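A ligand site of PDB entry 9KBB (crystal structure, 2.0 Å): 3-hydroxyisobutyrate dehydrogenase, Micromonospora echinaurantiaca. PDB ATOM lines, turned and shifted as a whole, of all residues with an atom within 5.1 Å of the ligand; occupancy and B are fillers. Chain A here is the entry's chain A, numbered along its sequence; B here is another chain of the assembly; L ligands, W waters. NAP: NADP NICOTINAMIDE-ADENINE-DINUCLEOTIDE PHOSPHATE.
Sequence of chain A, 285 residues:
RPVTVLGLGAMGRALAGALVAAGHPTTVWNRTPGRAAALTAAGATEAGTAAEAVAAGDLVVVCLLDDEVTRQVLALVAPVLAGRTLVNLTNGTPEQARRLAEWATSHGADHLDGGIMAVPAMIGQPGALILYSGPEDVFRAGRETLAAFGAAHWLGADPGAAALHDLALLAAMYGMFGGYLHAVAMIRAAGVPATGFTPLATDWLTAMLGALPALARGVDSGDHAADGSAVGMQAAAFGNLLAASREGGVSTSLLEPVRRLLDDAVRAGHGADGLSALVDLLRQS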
ATOM      1  N   GLY A   7     -19.419 -33.955  -2.701  1.00  0.00           N
ATOM      2  CA  GLY A   7     -20.243 -32.761  -2.680  1.00  0.00           C
ATOM      3  C   GLY A   7     -20.019 -31.894  -3.899  1.00  0.00           C
ATOM      4  O   GLY A   7     -18.906 -31.389  -4.109  1.00  0.00           O
ATOM      5  N   LEU A   8     -21.057 -31.717  -4.706  1.00  0.00           N
ATOM      6  CA  LEU A   8     -20.961 -30.939  -5.942  1.00  0.00           C
ATOM      7  C   LEU A   8     -21.974 -29.802  -5.965  1.00  0.00           C
ATOM      8  O   LEU A   8     -22.637 -29.548  -6.972  1.00  0.00           O
ATOM      9  CB  LEU A   8     -21.120 -31.838  -7.168  1.00  0.00           C
ATOM     10  CG  LEU A   8     -20.051 -32.912  -7.282  1.00  0.00           C
ATOM     11  CD1 LEU A   8     -20.354 -33.850  -8.443  1.00  0.00           C
ATOM     12  CD2 LEU A   8     -18.675 -32.283  -7.426  1.00  0.00           C
ATOM     13  N   GLY A   9     -22.100 -29.094  -4.855  1.00  0.00           N
ATOM     14  CA  GLY A   9     -22.763 -27.813  -4.859  1.00  0.00           C
ATOM     15  C   GLY A   9     -21.900 -26.784  -5.543  1.00  0.00           C
ATOM     16  O   GLY A   9     -20.960 -27.130  -6.253  1.00  0.00           O
ATOM     17  N   ALA A  10     -22.194 -25.492  -5.333  1.00  0.00           N
ATOM     18  CA  ALA A  10     -21.413 -24.441  -5.987  1.00  0.00           C
ATOM     19  C   ALA A  10     -19.933 -24.556  -5.630  1.00  0.00           C
ATOM     20  O   ALA A  10     -19.070 -24.556  -6.527  1.00  0.00           O
ATOM     21  CB  ALA A  10     -21.957 -23.064  -5.580  1.00  0.00           C
ATOM     22  N   MET A  11     -19.618 -24.676  -4.341  1.00  0.00           N
ATOM     23  CA  MET A  11     -18.226 -24.721  -3.916  1.00  0.00           C
ATOM     24  C   MET A  11     -17.572 -26.039  -4.303  1.00  0.00           C
ATOM     25  O   MET A  11     -16.440 -26.060  -4.780  1.00  0.00           O
ATOM     26  CB  MET A  11     -18.136 -24.508  -2.397  1.00  0.00           C
ATOM     27  CG  MET A  11     -16.730 -24.326  -1.868  1.00  0.00           C
ATOM     28  SD  MET A  11     -15.759 -23.106  -2.776  1.00  0.00           S
ATOM     29  CE  MET A  11     -16.215 -21.598  -1.925  1.00  0.00           C
ATOM     30  N   GLY A  12     -18.284 -27.157  -4.115  1.00  0.00           N
ATOM     31  CA  GLY A  12     -17.715 -28.455  -4.442  1.00  0.00           C
ATOM     32  C   GLY A  12     -17.351 -28.579  -5.909  1.00  0.00           C
ATOM     33  O   GLY A  12     -16.317 -29.164  -6.250  1.00  0.00           O
ATOM     34  N   TRP A  29     -18.400 -37.367  -6.355  1.00  0.00           N
ATOM     35  CA  TRP A  29     -19.688 -37.941  -6.005  1.00  0.00           C
ATOM     36  C   TRP A  29     -20.605 -36.842  -5.489  1.00  0.00           C
ATOM     37  O   TRP A  29     -20.148 -35.851  -4.906  1.00  0.00           O
ATOM     38  CB  TRP A  29     -19.563 -39.044  -4.948  1.00  0.00           C
ATOM     39  CG  TRP A  29     -20.896 -39.499  -4.431  1.00  0.00           C
ATOM     40  CD1 TRP A  29     -21.700 -40.477  -4.967  1.00  0.00           C
ATOM     41  CD2 TRP A  29     -21.605 -38.998  -3.290  1.00  0.00           C
ATOM     42  NE1 TRP A  29     -22.845 -40.611  -4.224  1.00  0.00           N
ATOM     43  CE2 TRP A  29     -22.815 -39.711  -3.192  1.00  0.00           C
ATOM     44  CE3 TRP A  29     -21.328 -38.005  -2.335  1.00  0.00           C
ATOM     45  CZ2 TRP A  29     -23.744 -39.471  -2.181  1.00  0.00           C
ATOM     46  CZ3 TRP A  29     -22.253 -37.767  -1.337  1.00  0.00           C
ATOM     47  CH2 TRP A  29     -23.451 -38.497  -1.262  1.00  0.00           C
ATOM     48  N   ASN A  30     -21.896 -37.035  -5.718  1.00  0.00           N
ATOM     49  CA  ASN A  30     -22.906 -36.119  -5.229  1.00  0.00           C
ATOM     50  C   ASN A  30     -24.200 -36.898  -5.056  1.00  0.00           C
ATOM     51  O   ASN A  30     -24.458 -37.867  -5.774  1.00  0.00           O
ATOM     52  CB  ASN A  30     -23.108 -34.936  -6.178  1.00  0.00           C
ATOM     53  CG  ASN A  30     -23.965 -33.843  -5.573  1.00  0.00           C
ATOM     54  OD1 ASN A  30     -23.567 -33.183  -4.620  1.00  0.00           O
ATOM     55  ND2 ASN A  30     -25.152 -33.666  -6.129  1.00  0.00           N
ATOM     56  N   ARG A  31     -24.995 -36.495  -4.054  1.00  0.00           N
ATOM     57  CA  ARG A  31     -26.263 -37.154  -3.790  1.00  0.00           C
ATOM     58  C   ARG A  31     -27.188 -37.084  -5.008  1.00  0.00           C
ATOM     59  O   ARG A  31     -27.642 -38.117  -5.526  1.00  0.00           O
ATOM     60  CB  ARG A  31     -26.930 -36.530  -2.570  1.00  0.00           C
ATOM     61  CG  ARG A  31     -28.412 -36.855  -2.425  1.00  0.00           C
ATOM     62  CD  ARG A  31     -29.020 -36.147  -1.239  1.00  0.00           C
ATOM     63  NE  ARG A  31     -29.053 -34.697  -1.417  1.00  0.00           N
ATOM     64  CZ  ARG A  31     -29.757 -33.868  -0.654  1.00  0.00           C
ATOM     65  NH1 ARG A  31     -30.478 -34.309   0.354  1.00  0.00           N
ATOM     66  NH2 ARG A  31     -29.736 -32.570  -0.920  1.00  0.00           N
ATOM     67  N   THR A  32     -27.452 -35.882  -5.476  1.00  0.00           N
ATOM     68  CA  THR A  32     -28.356 -35.697  -6.611  1.00  0.00           C
ATOM     69  C   THR A  32     -27.606 -35.838  -7.920  1.00  0.00           C
ATOM     70  O   THR A  32     -26.556 -35.208  -8.099  1.00  0.00           O
ATOM     71  CB  THR A  32     -29.010 -34.316  -6.554  1.00  0.00           C
ATOM     72  OG1 THR A  32     -29.731 -34.191  -5.316  1.00  0.00           O
ATOM     73  CG2 THR A  32     -29.971 -34.148  -7.725  1.00  0.00           C
ATOM     74  N   ARG A  35     -24.884 -33.300 -11.665  1.00  0.00           N
ATOM     75  CA  ARG A  35     -24.060 -32.184 -11.244  1.00  0.00           C
ATOM     76  C   ARG A  35     -22.624 -32.302 -11.727  1.00  0.00           C
ATOM     77  O   ARG A  35     -21.826 -31.376 -11.508  1.00  0.00           O
ATOM     78  CB  ARG A  35     -24.136 -32.089  -9.715  1.00  0.00           C
ATOM     79  CG  ARG A  35     -25.576 -31.787  -9.351  1.00  0.00           C
ATOM     80  CD  ARG A  35     -25.917 -30.437  -9.915  1.00  0.00           C
ATOM     81  NE  ARG A  35     -25.943 -29.420  -8.879  1.00  0.00           N
ATOM     82  CZ  ARG A  35     -26.591 -28.269  -8.988  1.00  0.00           C
ATOM     83  NH1 ARG A  35     -26.835 -27.736 -10.182  1.00  0.00           N
ATOM     84  NH2 ARG A  35     -26.963 -27.616  -7.881  1.00  0.00           N
ATOM     85  N   CYS A  63     -17.019 -31.273   0.804  1.00  0.00           N
ATOM     86  CA  CYS A  63     -17.616 -29.939   0.769  1.00  0.00           C
ATOM     87  C   CYS A  63     -19.128 -30.112   0.632  1.00  0.00           C
ATOM     88  O   CYS A  63     -19.695 -30.012  -0.456  1.00  0.00           O
ATOM     89  CB  CYS A  63     -17.046 -29.085  -0.352  1.00  0.00           C
ATOM     90  SG  CYS A  63     -17.531 -27.355  -0.236  1.00  0.00           S
ATOM     91  N   LEU A  64     -19.778 -30.390   1.757  1.00  0.00           N
ATOM     92  CA  LEU A  64     -21.218 -30.569   1.783  1.00  0.00           C
ATOM     93  C   LEU A  64     -21.893 -29.351   2.405  1.00  0.00           C
ATOM     94  O   LEU A  64     -21.257 -28.311   2.649  1.00  0.00           O
ATOM     95  CB  LEU A  64     -21.563 -31.870   2.513  1.00  0.00           C
ATOM     96  CG  LEU A  64     -20.954 -33.107   1.860  1.00  0.00           C
ATOM     97  CD1 LEU A  64     -20.952 -34.283   2.821  1.00  0.00           C
ATOM     98  CD2 LEU A  64     -21.706 -33.451   0.587  1.00  0.00           C
ATOM     99  N   LEU A  65     -23.192 -29.462   2.664  1.00  0.00           N
ATOM    100  CA  LEU A  65     -23.965 -28.305   3.103  1.00  0.00           C
ATOM    101  C   LEU A  65     -23.571 -27.861   4.503  1.00  0.00           C
ATOM    102  O   LEU A  65     -23.402 -26.665   4.764  1.00  0.00           O
ATOM    103  CB  LEU A  65     -25.456 -28.630   3.030  1.00  0.00           C
ATOM    104  CG  LEU A  65     -26.455 -27.573   3.538  1.00  0.00           C
ATOM    105  CD1 LEU A  65     -26.457 -26.344   2.648  1.00  0.00           C
ATOM    106  CD2 LEU A  65     -27.847 -28.185   3.627  1.00  0.00           C
ATOM    107  N   ASP A  66     -23.389 -28.811   5.414  1.00  0.00           N
ATOM    108  CA  ASP A  66     -23.104 -28.480   6.803  1.00  0.00           C
ATOM    109  C   ASP A  66     -22.470 -29.684   7.481  1.00  0.00           C
ATOM    110  O   ASP A  66     -22.336 -30.762   6.887  1.00  0.00           O
ATOM    111  CB  ASP A  66     -24.377 -28.013   7.521  1.00  0.00           C
ATOM    112  CG  ASP A  66     -25.516 -29.008   7.372  1.00  0.00           C
ATOM    113  OD1 ASP A  66     -25.365 -30.177   7.788  1.00  0.00           O
ATOM    114  OD2 ASP A  66     -26.573 -28.610   6.836  1.00  0.00           O
ATOM    115  N   VAL A  69     -24.683 -33.000   7.684  1.00  0.00           N
ATOM    116  CA  VAL A  69     -24.644 -33.797   6.455  1.00  0.00           C
ATOM    117  C   VAL A  69     -23.282 -34.472   6.327  1.00  0.00           C
ATOM    118  O   VAL A  69     -23.201 -35.652   5.973  1.00  0.00           O
ATOM    119  CB  VAL A  69     -24.942 -32.904   5.224  1.00  0.00           C
ATOM    120  CG1 VAL A  69     -24.594 -33.639   3.947  1.00  0.00           C
ATOM    121  CG2 VAL A  69     -26.392 -32.462   5.226  1.00  0.00           C
ATOM    122  N   GLN A  72     -22.970 -37.539   8.424  1.00  0.00           N
ATOM    123  CA  GLN A  72     -23.809 -38.625   7.950  1.00  0.00           C
ATOM    124  C   GLN A  72     -23.157 -39.362   6.786  1.00  0.00           C
ATOM    125  O   GLN A  72     -23.032 -40.593   6.797  1.00  0.00           O
ATOM    126  CB  GLN A  72     -25.192 -38.098   7.545  1.00  0.00           C
ATOM    127  CG  GLN A  72     -25.861 -38.913   6.432  1.00  0.00           C
ATOM    128  CD  GLN A  72     -26.959 -38.136   5.721  1.00  0.00           C
ATOM    129  OE1 GLN A  72     -28.009 -37.873   6.296  1.00  0.00           O
ATOM    130  NE2 GLN A  72     -26.715 -37.782   4.462  1.00  0.00           N
ATOM    131  N   VAL A  73     -22.721 -38.610   5.765  1.00  0.00           N
ATOM    132  CA  VAL A  73     -22.066 -39.215   4.604  1.00  0.00           C
ATOM    133  C   VAL A  73     -20.835 -39.985   5.042  1.00  0.00           C
ATOM    134  O   VAL A  73     -20.593 -41.112   4.580  1.00  0.00           O
ATOM    135  CB  VAL A  73     -21.722 -38.133   3.572  1.00  0.00           C
ATOM    136  CG1 VAL A  73     -20.998 -38.739   2.388  1.00  0.00           C
ATOM    137  CG2 VAL A  73     -22.974 -37.420   3.104  1.00  0.00           C
ATOM    138  N   LEU A  89     -13.554 -29.374   3.795  1.00  0.00           N
ATOM    139  CA  LEU A  89     -13.721 -27.982   3.397  1.00  0.00           C
ATOM    140  C   LEU A  89     -15.143 -27.469   3.626  1.00  0.00           C
ATOM    141  O   LEU A  89     -15.438 -26.334   3.258  1.00  0.00           O
ATOM    142  CB  LEU A  89     -13.314 -27.790   1.936  1.00  0.00           C
ATOM    143  CG  LEU A  89     -11.843 -28.104   1.653  1.00  0.00           C
ATOM    144  CD1 LEU A  89     -11.461 -27.646   0.265  1.00  0.00           C
ATOM    145  CD2 LEU A  89     -10.948 -27.462   2.693  1.00  0.00           C
ATOM    146  N   THR A  90     -16.013 -28.291   4.191  1.00  0.00           N
ATOM    147  CA  THR A  90     -17.300 -27.798   4.675  1.00  0.00           C
ATOM    148  C   THR A  90     -17.062 -26.825   5.822  1.00  0.00           C
ATOM    149  O   THR A  90     -16.184 -27.062   6.663  1.00  0.00           O
ATOM    150  CB  THR A  90     -18.178 -28.964   5.130  1.00  0.00           C
ATOM    151  OG1 THR A  90     -18.275 -29.952   4.101  1.00  0.00           O
ATOM    152  CG2 THR A  90     -19.578 -28.459   5.484  1.00  0.00           C
ATOM    153  N   ASN A  91     -17.814 -25.736   5.849  1.00  0.00           N
ATOM    154  CA  ASN A  91     -17.683 -24.794   6.955  1.00  0.00           C
ATOM    155  C   ASN A  91     -18.246 -25.406   8.228  1.00  0.00           C
ATOM    156  O   ASN A  91     -19.226 -26.159   8.202  1.00  0.00           O
ATOM    157  CB  ASN A  91     -18.407 -23.487   6.626  1.00  0.00           C
ATOM    158  CG  ASN A  91     -17.513 -22.494   5.908  1.00  0.00           C
ATOM    159  OD1 ASN A  91     -16.294 -22.595   5.963  1.00  0.00           O
ATOM    160  ND2 ASN A  91     -18.130 -21.532   5.223  1.00  0.00           N
ATOM    161  N   ILE A 116     -12.589 -22.159   3.801  1.00  0.00           N
ATOM    162  CA  ILE A 116     -12.421 -21.486   2.516  1.00  0.00           C
ATOM    163  C   ILE A 116     -12.739 -20.006   2.668  1.00  0.00           C
ATOM    164  O   ILE A 116     -13.868 -19.637   3.045  1.00  0.00           O
ATOM    165  CB  ILE A 116     -13.295 -22.136   1.432  1.00  0.00           C
ATOM    166  CG1 ILE A 116     -12.932 -23.614   1.294  1.00  0.00           C
ATOM    167  CG2 ILE A 116     -13.162 -21.400   0.112  1.00  0.00           C
ATOM    168  CD1 ILE A 116     -14.001 -24.438   0.601  1.00  0.00           C
ATOM    169  N   ALA A 118     -12.637 -17.775   0.140  1.00  0.00           N
ATOM    170  CA  ALA A 118     -12.822 -17.228  -1.200  1.00  0.00           C
ATOM    171  C   ALA A 118     -14.147 -17.704  -1.762  1.00  0.00           C
ATOM    172  O   ALA A 118     -14.774 -18.647  -1.248  1.00  0.00           O
ATOM    173  CB  ALA A 118     -11.676 -17.629  -2.129  1.00  0.00           C
ATOM    174  N   VAL A 119     -14.586 -17.043  -2.830  1.00  0.00           N
ATOM    175  CA  VAL A 119     -15.826 -17.379  -3.518  1.00  0.00           C
ATOM    176  C   VAL A 119     -15.542 -18.504  -4.504  1.00  0.00           C
ATOM    177  O   VAL A 119     -14.388 -18.653  -4.947  1.00  0.00           O
ATOM    178  CB  VAL A 119     -16.430 -16.161  -4.222  1.00  0.00           C
ATOM    179  CG1 VAL A 119     -16.855 -15.101  -3.209  1.00  0.00           C
ATOM    180  CG2 VAL A 119     -15.450 -15.586  -5.221  1.00  0.00           C
ATOM    181  N   PRO A 120     -16.548 -19.308  -4.876  1.00  0.00           N
ATOM    182  CA  PRO A 120     -16.337 -20.391  -5.851  1.00  0.00           C
ATOM    183  C   PRO A 120     -15.614 -19.961  -7.115  1.00  0.00           C
ATOM    184  O   PRO A 120     -14.744 -20.687  -7.616  1.00  0.00           O
ATOM    185  CB  PRO A 120     -17.767 -20.845  -6.161  1.00  0.00           C
ATOM    186  CG  PRO A 120     -18.459 -20.677  -4.848  1.00  0.00           C
ATOM    187  CD  PRO A 120     -17.907 -19.364  -4.305  1.00  0.00           C
ATOM    188  N   GLY B 228     -20.439 -13.205  -6.385  1.00  0.00           N
ATOM    189  CA  GLY B 228     -20.382 -14.580  -5.966  1.00  0.00           C
ATOM    190  C   GLY B 228     -20.678 -14.753  -4.497  1.00  0.00           C
ATOM    191  O   GLY B 228     -21.186 -15.805  -4.093  1.00  0.00           O
ATOM    192  N   MET B 233     -25.923 -16.988   1.037  1.00  0.00           N
ATOM    193  CA  MET B 233     -24.853 -17.836   1.522  1.00  0.00           C
ATOM    194  C   MET B 233     -24.223 -17.240   2.773  1.00  0.00           C
ATOM    195  O   MET B 233     -23.935 -17.951   3.745  1.00  0.00           O
ATOM    196  CB  MET B 233     -23.796 -18.049   0.437  1.00  0.00           C
ATOM    197  CG  MET B 233     -22.494 -18.682   0.930  1.00  0.00           C
ATOM    198  SD  MET B 233     -21.225 -17.512   1.471  1.00  0.00           S
ATOM    199  CE  MET B 233     -21.199 -16.362   0.105  1.00  0.00           C
ATOM    200  N   ALA B 237     -23.795 -18.835   6.448  1.00  0.00           N
ATOM    201  CA  ALA B 237     -22.490 -19.045   7.080  1.00  0.00           C
ATOM    202  C   ALA B 237     -22.369 -18.328   8.420  1.00  0.00           C
ATOM    203  O   ALA B 237     -21.468 -18.650   9.200  1.00  0.00           O
ATOM    204  CB  ALA B 237     -21.374 -18.580   6.146  1.00  0.00           C
HETATM  205  PA  NAP L   1     -24.664 -25.620  -2.093  1.00  0.00           P
HETATM  206  O1A NAP L   1     -25.954 -25.410  -1.381  1.00  0.00           O
HETATM  207  O2A NAP L   1     -24.522 -25.121  -3.484  1.00  0.00           O
HETATM  208  O5B NAP L   1     -24.275 -27.175  -2.049  1.00  0.00           O
HETATM  209  C5B NAP L   1     -24.579 -28.003  -0.904  1.00  0.00           C
HETATM  210  C4B NAP L   1     -24.103 -29.409  -1.164  1.00  0.00           C
HETATM  211  O4B NAP L   1     -24.518 -30.273  -0.068  1.00  0.00           O
HETATM  212  C3B NAP L   1     -24.637 -30.088  -2.438  1.00  0.00           C
HETATM  213  O3B NAP L   1     -23.610 -30.811  -3.104  1.00  0.00           O
HETATM  214  C2B NAP L   1     -25.737 -31.012  -1.919  1.00  0.00           C
HETATM  215  O2B NAP L   1     -25.904 -32.167  -2.734  1.00  0.00           O
HETATM  216  C1B NAP L   1     -25.113 -31.435  -0.596  1.00  0.00           C
HETATM  217  N9A NAP L   1     -26.071 -31.973   0.355  1.00  0.00           N
HETATM  218  C8A NAP L   1     -27.034 -31.272   1.039  1.00  0.00           C
HETATM  219  N7A NAP L   1     -27.750 -32.034   1.836  1.00  0.00           N
HETATM  220  C5A NAP L   1     -27.223 -33.301   1.655  1.00  0.00           C
HETATM  221  C6A NAP L   1     -27.553 -34.546   2.222  1.00  0.00           C
HETATM  222  N6A NAP L   1     -28.525 -34.718   3.108  1.00  0.00           N
HETATM  223  N1A NAP L   1     -26.817 -35.624   1.842  1.00  0.00           N
HETATM  224  C2A NAP L   1     -25.841 -35.442   0.947  1.00  0.00           C
HETATM  225  N3A NAP L   1     -25.447 -34.322   0.350  1.00  0.00           N
HETATM  226  C4A NAP L   1     -26.188 -33.273   0.751  1.00  0.00           C
HETATM  227  O3  NAP L   1     -23.497 -24.966  -1.208  1.00  0.00           O
HETATM  228  PN  NAP L   1     -21.965 -24.622  -1.563  1.00  0.00           P
HETATM  229  O1N NAP L   1     -21.385 -25.777  -2.294  1.00  0.00           O
HETATM  230  O2N NAP L   1     -21.893 -23.288  -2.221  1.00  0.00           O
HETATM  231  O5D NAP L   1     -21.333 -24.526  -0.101  1.00  0.00           O
HETATM  232  C5D NAP L   1     -20.756 -25.744   0.433  1.00  0.00           C
HETATM  233  C4D NAP L   1     -19.855 -25.400   1.600  1.00  0.00           C
HETATM  234  O4D NAP L   1     -18.870 -24.431   1.178  1.00  0.00           O
HETATM  235  C3D NAP L   1     -20.556 -24.810   2.835  1.00  0.00           C
HETATM  236  O3D NAP L   1     -20.102 -25.448   4.025  1.00  0.00           O
HETATM  237  C2D NAP L   1     -20.153 -23.343   2.752  1.00  0.00           C
HETATM  238  O2D NAP L   1     -20.150 -22.680   4.008  1.00  0.00           O
HETATM  239  C1D NAP L   1     -18.752 -23.438   2.167  1.00  0.00           C
HETATM  240  N1N NAP L   1     -18.311 -22.164   1.520  1.00  0.00           N
HETATM  241  C2N NAP L   1     -19.021 -21.626   0.483  1.00  0.00           C
HETATM  242  C3N NAP L   1     -18.762 -20.390  -0.027  1.00  0.00           C
HETATM  243  C7N NAP L   1     -19.558 -19.942  -1.183  1.00  0.00           C
HETATM  244  O7N NAP L   1     -19.620 -18.738  -1.472  1.00  0.00           O
HETATM  245  N7N NAP L   1     -20.184 -20.863  -1.892  1.00  0.00           N
HETATM  246  C4N NAP L   1     -17.659 -19.586   0.583  1.00  0.00           C
HETATM  247  C5N NAP L   1     -16.919 -20.277   1.640  1.00  0.00           C
HETATM  248  C6N NAP L   1     -17.189 -21.515   1.987  1.00  0.00           C
HETATM  249  P2B NAP L   1     -27.213 -32.149  -3.684  1.00  0.00           P
HETATM  250  O1X NAP L   1     -26.793 -31.610  -5.029  1.00  0.00           O
HETATM  251  O2X NAP L   1     -28.242 -31.291  -3.002  1.00  0.00           O
HETATM  252  O3X NAP L   1     -27.625 -33.591  -3.757  1.00  0.00           O
HETATM  253  O   HOH W   1     -28.222 -28.596  -3.100  1.00  0.00           O
HETATM  254  O   HOH W   2     -25.778 -24.721  -5.754  1.00  0.00           O
HETATM  255  O   HOH W   3     -20.468 -28.233  -2.399  1.00  0.00           O
HETATM  256  O   HOH W   4     -20.250 -19.707   2.924  1.00  0.00           O
HETATM  257  O   HOH W   5     -24.023 -34.470  -2.144  1.00  0.00           O
HETATM  258  O   HOH W   6     -21.774 -19.063  -4.185  1.00  0.00           O
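An oxygen (O7N) of the ligand lies close to the side-chain sulfur (SD) of Met 233 of chain B, 3.6 Å away.
Residues that only touch the ligand: Gly 7 (3.8 Å), Gly 12 (3.9 Å), Val 69 (3.5 Å), Thr 90 (3.4 Å), Ile 116 (3.4 Å), Ala 118 (3.5 Å) and Pro 120 (3.4 Å).
Hydrophobic or aromatic side chains that line the ligand: Ala 10, Met 11, Leu 64, Leu 65, Val 69, Ile 116, Pro 120 and Met 233 of chain B.
Of the 28 residues printed, 20 come within 4 Å of the ligand.
The nearest printed residue that does not touch the ligand is Val 73 (4.1 Å).
Water W3 lies within hydrogen-bond range of an oxygen (O1N) of the ligand, the backbone carbonyl oxygen (O) of Cys 63, the backbone NH (N) of Gly 12 and the backbone NH (N) of Gly 9.
Water W5 lies within hydrogen-bond range of OD1 of Asn 30 (2.8 Å), N3A of the ligand (2.9 Å) and N of Arg 31 (2.9 Å).
Water W4 lies within hydrogen-bond range of the side-chain sulfur of Met 233 of chain B and an oxygen (O2D) of the ligand.
Water W6 lies within hydrogen-bond range of the backbone carbonyl oxygen of Gly 228 of chain B and a nitrogen (N7N) of the ligand.
The backbone carbonyl oxygen (O) of Thr 32 sits at hydrogen-bond distance from the side-chain amide nitrogen (ND2) of Asn 30 (2.9 Å).
The side-chain amide oxygen of Asn 30 lies within hydrogen-bond range of the backbone NH of Leu 8 (2.9 Å).
The side-chain hydroxyl of Thr 90 is in hydrogen-bond range of the backbone NH of Leu 64, at 2.8 Å.
The side-chain carboxylate of Asp 66 is in hydrogen-bond range of the backbone NH of Val 69.
O of Trp 29 sits at hydrogen-bond distance from N of Gly 7, 3.0 Å away.
The backbone NH of Asn 91 sits at hydrogen-bond distance from an oxygen (O3D) of the ligand, at 2.9 Å.
ND2 of Asn 91 lies within hydrogen-bond range of O2D of the ligand (2.6 Å).
O3X of the ligand lies within hydrogen-bond range of N of Thr 32 (2.9 Å).
An oxygen (O3X) of the ligand sits at hydrogen-bond distance from the side-chain hydroxyl (OG1) of Thr 32 (2.7 Å).
The side-chain amide oxygen (OD1) of Asn 30 is in hydrogen-bond range of an oxygen (O3B) of the ligand.
An oxygen (O2X) of the ligand is in salt-bridge range of the guanidinium group (NH2) of Arg 31, 2.9 Å away.
N of Gly 9 lies within hydrogen-bond range of O3B of the ligand (2.9 Å).
The backbone NH of Met 11 sits at hydrogen-bond distance from an oxygen (O1N) of the ligand.
O2A of the ligand lies within hydrogen-bond range of N of Ala 10 (3.0 Å).
The backbone NH of Leu 65 lies within hydrogen-bond range of an oxygen (O4B) of the ligand (3.1 Å).
N of Leu 8 sits at hydrogen-bond distance from O3B of the ligand, at 3.1 Å.
The backbone carbonyl oxygen of Leu 64 is in hydrogen-bond range of an oxygen (O3D) of the ligand (3.4 Å).
The side-chain amide nitrogen of Gln 72 sits at hydrogen-bond distance from a nitrogen (N1A) of the ligand, at 3.4 Å.
The side-chain sulfur (SG) of Cys 63 lies within hydrogen-bond range of an oxygen (O4D) of the ligand.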
